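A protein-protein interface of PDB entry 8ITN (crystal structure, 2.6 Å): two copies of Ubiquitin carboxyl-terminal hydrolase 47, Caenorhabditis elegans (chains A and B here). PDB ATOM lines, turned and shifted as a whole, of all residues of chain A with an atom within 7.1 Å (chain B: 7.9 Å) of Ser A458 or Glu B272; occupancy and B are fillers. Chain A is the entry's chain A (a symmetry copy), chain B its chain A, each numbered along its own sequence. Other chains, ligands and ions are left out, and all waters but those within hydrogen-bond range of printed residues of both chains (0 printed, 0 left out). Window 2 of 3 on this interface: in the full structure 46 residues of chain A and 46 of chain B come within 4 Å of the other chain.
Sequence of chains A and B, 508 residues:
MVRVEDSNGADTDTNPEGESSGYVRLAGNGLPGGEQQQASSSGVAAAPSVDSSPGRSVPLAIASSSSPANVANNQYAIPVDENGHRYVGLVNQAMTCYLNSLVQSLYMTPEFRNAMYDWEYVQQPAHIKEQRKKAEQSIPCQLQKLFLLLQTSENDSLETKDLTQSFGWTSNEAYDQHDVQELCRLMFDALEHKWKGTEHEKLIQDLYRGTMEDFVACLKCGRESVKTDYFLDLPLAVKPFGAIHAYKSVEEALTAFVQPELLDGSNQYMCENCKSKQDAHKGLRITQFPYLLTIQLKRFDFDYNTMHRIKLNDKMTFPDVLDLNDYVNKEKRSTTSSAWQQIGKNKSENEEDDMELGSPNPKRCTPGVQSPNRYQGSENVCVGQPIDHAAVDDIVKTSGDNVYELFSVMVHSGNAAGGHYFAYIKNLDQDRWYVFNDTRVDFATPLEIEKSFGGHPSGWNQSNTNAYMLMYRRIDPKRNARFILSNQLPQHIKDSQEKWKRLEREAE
The backbone carbonyl oxygen (O) of Ser A458 lies close to the side-chain hydroxyl (OH) of Tyr B269, 2.2 Å away.
OE1 of Glu B272 sits at hydrogen-bond distance from OG of Ser A458.
The backbone carbonyl oxygen (O) of Tyr B269 is in hydrogen-bond range of the backbone NH (N) of Gln B278, 2.8 Å away.
The backbone carbonyl oxygen (O) of Val B216 is in hydrogen-bond range of the backbone NH (N) of Ser B225.
O of His A456 touches N of Met B270, at 3.5 Å.
Pro A457 touches Tyr B269 (O to CE1, 3.1 Å).
Met B270 touches Pro A457.
Met B270 touches Ser A458 (O to CA, 3.2 Å).
O of Ser B225 touches CH2 of Trp A460, 3.6 Å away.
Ser A458 touches three residues of chain B.
Glu B272 touches one residue of chain A.
Of the printed residues of chain A, Tyr B269 touches Pro A457 (3.1 Å) and Ser A458 (2.2 Å).
Of the printed residues of chain B, Pro A457 touches Tyr B269 and Met B270.
Of the printed residues of chain A, Ser B225 touches Trp A460 (3.6 Å).
Of the printed residues of chain B, Trp A460 touches Ser B225.
Asn A461 touches none of the printed residues of chain B.
The nearest printed residue of chain B that does not touch His A456 is Tyr B269 (4.2 Å).
Printed residues of chain B that touch a printed residue of chain A: Ser B225, Tyr B269, Met B270 and Glu B272.
No position is printed for both chains.
Of the 7 pairs that touch across the chains among the printed residues, none has its exchanged pair printed and touching as well.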
ATOM      1  N   GLY A 455     -18.900  28.745   1.518  1.00  0.00           N
ATOM      2  CA  GLY A 455     -17.470  28.917   1.673  1.00  0.00           C
ATOM      3  C   GLY A 455     -16.767  27.577   1.696  1.00  0.00           C
ATOM      4  O   GLY A 455     -17.268  26.619   2.294  1.00  0.00           O
ATOM      5  N   HIS A 456     -15.614  27.491   1.047  1.00  0.00           N
ATOM      6  CA  HIS A 456     -14.918  26.217   0.932  1.00  0.00           C
ATOM      7  C   HIS A 456     -14.261  25.851   2.257  1.00  0.00           C
ATOM      8  O   HIS A 456     -13.415  26.607   2.748  1.00  0.00           O
ATOM      9  CB  HIS A 456     -13.876  26.279  -0.175  1.00  0.00           C
ATOM     10  CG  HIS A 456     -14.465  26.270  -1.550  1.00  0.00           C
ATOM     11  ND1 HIS A 456     -14.757  25.104  -2.226  1.00  0.00           N
ATOM     12  CD2 HIS A 456     -14.829  27.282  -2.371  1.00  0.00           C
ATOM     13  CE1 HIS A 456     -15.269  25.399  -3.407  1.00  0.00           C
ATOM     14  NE2 HIS A 456     -15.323  26.714  -3.520  1.00  0.00           N
ATOM     15  N   PRO A 457     -14.617  24.715   2.866  1.00  0.00           N
ATOM     16  CA  PRO A 457     -13.956  24.301   4.111  1.00  0.00           C
ATOM     17  C   PRO A 457     -12.545  23.787   3.870  1.00  0.00           C
ATOM     18  O   PRO A 457     -11.982  23.987   2.790  1.00  0.00           O
ATOM     19  CB  PRO A 457     -14.879  23.199   4.645  1.00  0.00           C
ATOM     20  CG  PRO A 457     -15.523  22.637   3.427  1.00  0.00           C
ATOM     21  CD  PRO A 457     -15.696  23.791   2.476  1.00  0.00           C
ATOM     22  N   SER A 458     -11.971  23.115   4.870  1.00  0.00           N
ATOM     23  CA  SER A 458     -10.580  22.683   4.768  1.00  0.00           C
ATOM     24  C   SER A 458     -10.389  21.614   3.700  1.00  0.00           C
ATOM     25  O   SER A 458      -9.320  21.542   3.084  1.00  0.00           O
ATOM     26  CB  SER A 458     -10.089  22.177   6.123  1.00  0.00           C
ATOM     27  OG  SER A 458     -10.107  23.216   7.087  1.00  0.00           O
ATOM     28  N   GLY A 459     -11.399  20.783   3.464  1.00  0.00           N
ATOM     29  CA  GLY A 459     -11.297  19.754   2.449  1.00  0.00           C
ATOM     30  C   GLY A 459     -12.560  18.932   2.327  1.00  0.00           C
ATOM     31  O   GLY A 459     -13.668  19.479   2.330  1.00  0.00           O
ATOM     32  N   TRP A 460     -12.410  17.618   2.212  1.00  0.00           N
ATOM     33  CA  TRP A 460     -13.547  16.698   2.212  1.00  0.00           C
ATOM     34  C   TRP A 460     -13.771  16.119   3.603  1.00  0.00           C
ATOM     35  O   TRP A 460     -13.851  14.907   3.800  1.00  0.00           O
ATOM     36  CB  TRP A 460     -13.334  15.598   1.178  1.00  0.00           C
ATOM     37  CG  TRP A 460     -13.191  16.127  -0.218  1.00  0.00           C
ATOM     38  CD1 TRP A 460     -14.199  16.435  -1.086  1.00  0.00           C
ATOM     39  CD2 TRP A 460     -11.968  16.418  -0.907  1.00  0.00           C
ATOM     40  NE1 TRP A 460     -13.680  16.898  -2.272  1.00  0.00           N
ATOM     41  CE2 TRP A 460     -12.312  16.895  -2.187  1.00  0.00           C
ATOM     42  CE3 TRP A 460     -10.615  16.318  -0.565  1.00  0.00           C
ATOM     43  CZ2 TRP A 460     -11.353  17.274  -3.126  1.00  0.00           C
ATOM     44  CZ3 TRP A 460      -9.664  16.693  -1.499  1.00  0.00           C
ATOM     45  CH2 TRP A 460     -10.039  17.165  -2.763  1.00  0.00           C
ATOM     46  N   ASN A 461     -13.867  17.012   4.591  1.00  0.00           N
ATOM     47  CA  ASN A 461     -14.038  16.587   5.977  1.00  0.00           C
ATOM     48  C   ASN A 461     -15.396  15.919   6.205  1.00  0.00           C
ATOM     49  O   ASN A 461     -15.455  14.804   6.736  1.00  0.00           O
ATOM     50  CB  ASN A 461     -13.834  17.776   6.920  1.00  0.00           C
ATOM     51  CG  ASN A 461     -12.401  18.281   6.921  1.00  0.00           C
ATOM     52  OD1 ASN A 461     -11.541  17.746   6.221  1.00  0.00           O
ATOM     53  ND2 ASN A 461     -12.141  19.322   7.703  1.00  0.00           N
ATOM     54  N   GLN A 462     -16.504  16.579   5.850  1.00  0.00           N
ATOM     55  CA  GLN A 462     -16.544  17.941   5.312  1.00  0.00           C
ATOM     56  C   GLN A 462     -17.862  18.644   5.701  1.00  0.00           C
ATOM     57  O   GLN A 462     -18.691  18.966   4.850  1.00  0.00           O
ATOM     58  CB  GLN A 462     -16.382  17.924   3.792  1.00  0.00           C
ATOM     59  CG  GLN A 462     -17.672  17.656   3.034  1.00  0.00           C
ATOM     60  CD  GLN A 462     -17.913  16.178   2.797  1.00  0.00           C
ATOM     61  OE1 GLN A 462     -17.936  15.716   1.656  1.00  0.00           O
ATOM     62  NE2 GLN A 462     -18.096  15.429   3.878  1.00  0.00           N
ATOM     63  N   VAL B 216      -7.072  20.908  -4.455  1.00  0.00           N
ATOM     64  CA  VAL B 216      -7.143  22.252  -3.896  1.00  0.00           C
ATOM     65  C   VAL B 216      -5.721  22.635  -3.514  1.00  0.00           C
ATOM     66  O   VAL B 216      -5.138  22.033  -2.605  1.00  0.00           O
ATOM     67  CB  VAL B 216      -8.081  22.345  -2.686  1.00  0.00           C
ATOM     68  CG1 VAL B 216      -8.245  23.796  -2.268  1.00  0.00           C
ATOM     69  CG2 VAL B 216      -9.437  21.726  -3.003  1.00  0.00           C
ATOM     70  N   CYS B 218      -3.312  25.508  -2.129  1.00  0.00           N
ATOM     71  CA  CYS B 218      -3.190  26.800  -1.467  1.00  0.00           C
ATOM     72  C   CYS B 218      -2.112  27.631  -2.151  1.00  0.00           C
ATOM     73  O   CYS B 218      -0.996  27.153  -2.376  1.00  0.00           O
ATOM     74  CB  CYS B 218      -2.856  26.613   0.013  1.00  0.00           C
ATOM     75  SG  CYS B 218      -2.582  28.158   0.922  1.00  0.00           S
ATOM     76  N   CYS B 221       1.042  28.708   0.956  1.00  0.00           N
ATOM     77  CA  CYS B 221       2.017  27.706   1.370  1.00  0.00           C
ATOM     78  C   CYS B 221       2.370  26.721   0.264  1.00  0.00           C
ATOM     79  O   CYS B 221       3.438  26.103   0.328  1.00  0.00           O
ATOM     80  CB  CYS B 221       1.498  26.943   2.590  1.00  0.00           C
ATOM     81  SG  CYS B 221       0.095  25.861   2.254  1.00  0.00           S
ATOM     82  N   ARG B 223       0.790  23.885  -0.449  1.00  0.00           N
ATOM     83  CA  ARG B 223       0.348  22.525  -0.182  1.00  0.00           C
ATOM     84  C   ARG B 223      -0.940  22.215  -0.934  1.00  0.00           C
ATOM     85  O   ARG B 223      -1.770  23.095  -1.186  1.00  0.00           O
ATOM     86  CB  ARG B 223       0.141  22.316   1.318  1.00  0.00           C
ATOM     87  CG  ARG B 223       1.423  22.364   2.132  1.00  0.00           C
ATOM     88  CD  ARG B 223       2.246  21.101   1.942  1.00  0.00           C
ATOM     89  NE  ARG B 223       3.568  21.214   2.547  1.00  0.00           N
ATOM     90  CZ  ARG B 223       3.827  20.999   3.829  1.00  0.00           C
ATOM     91  NH1 ARG B 223       2.870  20.668   4.683  1.00  0.00           N
ATOM     92  NH2 ARG B 223       5.075  21.122   4.269  1.00  0.00           N
ATOM     93  N   SER B 225      -4.314  19.340  -1.518  1.00  0.00           N
ATOM     94  CA  SER B 225      -5.153  18.225  -1.093  1.00  0.00           C
ATOM     95  C   SER B 225      -5.793  17.652  -2.351  1.00  0.00           C
ATOM     96  O   SER B 225      -6.667  18.285  -2.951  1.00  0.00           O
ATOM     97  CB  SER B 225      -6.208  18.667  -0.081  1.00  0.00           C
ATOM     98  OG  SER B 225      -7.152  19.541  -0.672  1.00  0.00           O
ATOM     99  N   TYR B 269     -10.135  29.946   0.588  1.00  0.00           N
ATOM    100  CA  TYR B 269     -10.063  28.549   0.988  1.00  0.00           C
ATOM    101  C   TYR B 269      -9.444  28.442   2.373  1.00  0.00           C
ATOM    102  O   TYR B 269      -8.382  29.018   2.626  1.00  0.00           O
ATOM    103  CB  TYR B 269      -9.250  27.740  -0.025  1.00  0.00           C
ATOM    104  CG  TYR B 269      -8.906  26.341   0.427  1.00  0.00           C
ATOM    105  CD1 TYR B 269      -9.876  25.350   0.476  1.00  0.00           C
ATOM    106  CD2 TYR B 269      -7.606  26.008   0.792  1.00  0.00           C
ATOM    107  CE1 TYR B 269      -9.565  24.066   0.885  1.00  0.00           C
ATOM    108  CE2 TYR B 269      -7.284  24.730   1.201  1.00  0.00           C
ATOM    109  CZ  TYR B 269      -8.265  23.764   1.245  1.00  0.00           C
ATOM    110  OH  TYR B 269      -7.937  22.491   1.651  1.00  0.00           O
ATOM    111  N   MET B 270     -10.112  27.712   3.263  1.00  0.00           N
ATOM    112  CA  MET B 270      -9.606  27.477   4.615  1.00  0.00           C
ATOM    113  C   MET B 270      -8.463  26.475   4.538  1.00  0.00           C
ATOM    114  O   MET B 270      -8.684  25.263   4.489  1.00  0.00           O
ATOM    115  CB  MET B 270     -10.720  26.976   5.526  1.00  0.00           C
ATOM    116  CG  MET B 270     -11.206  28.004   6.533  1.00  0.00           C
ATOM    117  SD  MET B 270      -9.921  28.515   7.691  1.00  0.00           S
ATOM    118  CE  MET B 270      -9.486  26.941   8.426  1.00  0.00           C
ATOM    119  N   CYS B 271      -7.232  26.976   4.506  1.00  0.00           N
ATOM    120  CA  CYS B 271      -6.067  26.107   4.454  1.00  0.00           C
ATOM    121  C   CYS B 271      -5.762  25.574   5.846  1.00  0.00           C
ATOM    122  O   CYS B 271      -5.740  26.332   6.820  1.00  0.00           O
ATOM    123  CB  CYS B 271      -4.859  26.856   3.896  1.00  0.00           C
ATOM    124  SG  CYS B 271      -3.359  25.858   3.808  1.00  0.00           S
ATOM    125  N   GLU B 272      -5.542  24.262   5.938  1.00  0.00           N
ATOM    126  CA  GLU B 272      -5.220  23.661   7.226  1.00  0.00           C
ATOM    127  C   GLU B 272      -3.759  23.892   7.599  1.00  0.00           C
ATOM    128  O   GLU B 272      -3.442  24.088   8.778  1.00  0.00           O
ATOM    129  CB  GLU B 272      -5.542  22.168   7.201  1.00  0.00           C
ATOM    130  CG  GLU B 272      -5.356  21.461   8.538  1.00  0.00           C
ATOM    131  CD  GLU B 272      -6.428  21.817   9.557  1.00  0.00           C
ATOM    132  OE1 GLU B 272      -7.441  22.447   9.180  1.00  0.00           O
ATOM    133  OE2 GLU B 272      -6.257  21.458  10.739  1.00  0.00           O
ATOM    134  N   ASN B 273      -2.863  23.889   6.611  1.00  0.00           N
ATOM    135  CA  ASN B 273      -1.462  24.182   6.885  1.00  0.00           C
ATOM    136  C   ASN B 273      -1.274  25.643   7.272  1.00  0.00           C
ATOM    137  O   ASN B 273      -0.524  25.950   8.206  1.00  0.00           O
ATOM    138  CB  ASN B 273      -0.608  23.831   5.669  1.00  0.00           C
ATOM    139  CG  ASN B 273       0.874  23.938   5.952  1.00  0.00           C
ATOM    140  OD1 ASN B 273       1.306  23.824   7.098  1.00  0.00           O
ATOM    141  ND2 ASN B 273       1.662  24.159   4.909  1.00  0.00           N
ATOM    142  N   CYS B 274      -1.940  26.556   6.564  1.00  0.00           N
ATOM    143  CA  CYS B 274      -1.905  27.968   6.920  1.00  0.00           C
ATOM    144  C   CYS B 274      -2.826  28.307   8.084  1.00  0.00           C
ATOM    145  O   CYS B 274      -2.719  29.410   8.631  1.00  0.00           O
ATOM    146  CB  CYS B 274      -2.271  28.826   5.706  1.00  0.00           C
ATOM    147  SG  CYS B 274      -1.032  28.819   4.387  1.00  0.00           S
ATOM    148  N   LYS B 275      -3.721  27.392   8.466  1.00  0.00           N
ATOM    149  CA  LYS B 275      -4.629  27.582   9.600  1.00  0.00           C
ATOM    150  C   LYS B 275      -5.486  28.836   9.446  1.00  0.00           C
ATOM    151  O   LYS B 275      -5.911  29.435  10.437  1.00  0.00           O
ATOM    152  CB  LYS B 275      -3.860  27.619  10.924  1.00  0.00           C
ATOM    153  CG  LYS B 275      -3.295  26.274  11.348  1.00  0.00           C
ATOM    154  CD  LYS B 275      -4.394  25.345  11.838  1.00  0.00           C
ATOM    155  CE  LYS B 275      -3.880  23.927  12.019  1.00  0.00           C
ATOM    156  NZ  LYS B 275      -2.633  23.882  12.829  1.00  0.00           N
ATOM    157  N   SER B 276      -5.753  29.239   8.208  1.00  0.00           N
ATOM    158  CA  SER B 276      -6.524  30.445   7.941  1.00  0.00           C
ATOM    159  C   SER B 276      -7.011  30.398   6.498  1.00  0.00           C
ATOM    160  O   SER B 276      -6.680  29.486   5.736  1.00  0.00           O
ATOM    161  CB  SER B 276      -5.696  31.707   8.204  1.00  0.00           C
ATOM    162  OG  SER B 276      -4.520  31.716   7.412  1.00  0.00           O
ATOM    163  N   LYS B 277      -7.794  31.408   6.128  1.00  0.00           N
ATOM    164  CA  LYS B 277      -8.322  31.517   4.777  1.00  0.00           C
ATOM    165  C   LYS B 277      -7.279  32.143   3.862  1.00  0.00           C
ATOM    166  O   LYS B 277      -6.723  33.202   4.170  1.00  0.00           O
ATOM    167  CB  LYS B 277      -9.605  32.350   4.774  1.00  0.00           C
ATOM    168  CG  LYS B 277     -10.683  31.824   5.709  1.00  0.00           C
ATOM    169  CD  LYS B 277     -11.979  32.611   5.574  1.00  0.00           C
ATOM    170  CE  LYS B 277     -12.623  32.384   4.218  1.00  0.00           C
ATOM    171  NZ  LYS B 277     -13.944  33.062   4.114  1.00  0.00           N
ATOM    172  N   GLN B 278      -7.012  31.484   2.735  1.00  0.00           N
ATOM    173  CA  GLN B 278      -6.018  31.946   1.778  1.00  0.00           C
ATOM    174  C   GLN B 278      -6.551  31.757   0.367  1.00  0.00           C
ATOM    175  O   GLN B 278      -7.466  30.966   0.126  1.00  0.00           O
ATOM    176  CB  GLN B 278      -4.687  31.193   1.934  1.00  0.00           C
ATOM    177  CG  GLN B 278      -4.063  31.269   3.319  1.00  0.00           C
ATOM    178  CD  GLN B 278      -3.490  32.635   3.631  1.00  0.00           C
ATOM    179  OE1 GLN B 278      -3.230  33.434   2.731  1.00  0.00           O
ATOM    180  NE2 GLN B 278      -3.288  32.911   4.912  1.00  0.00           N
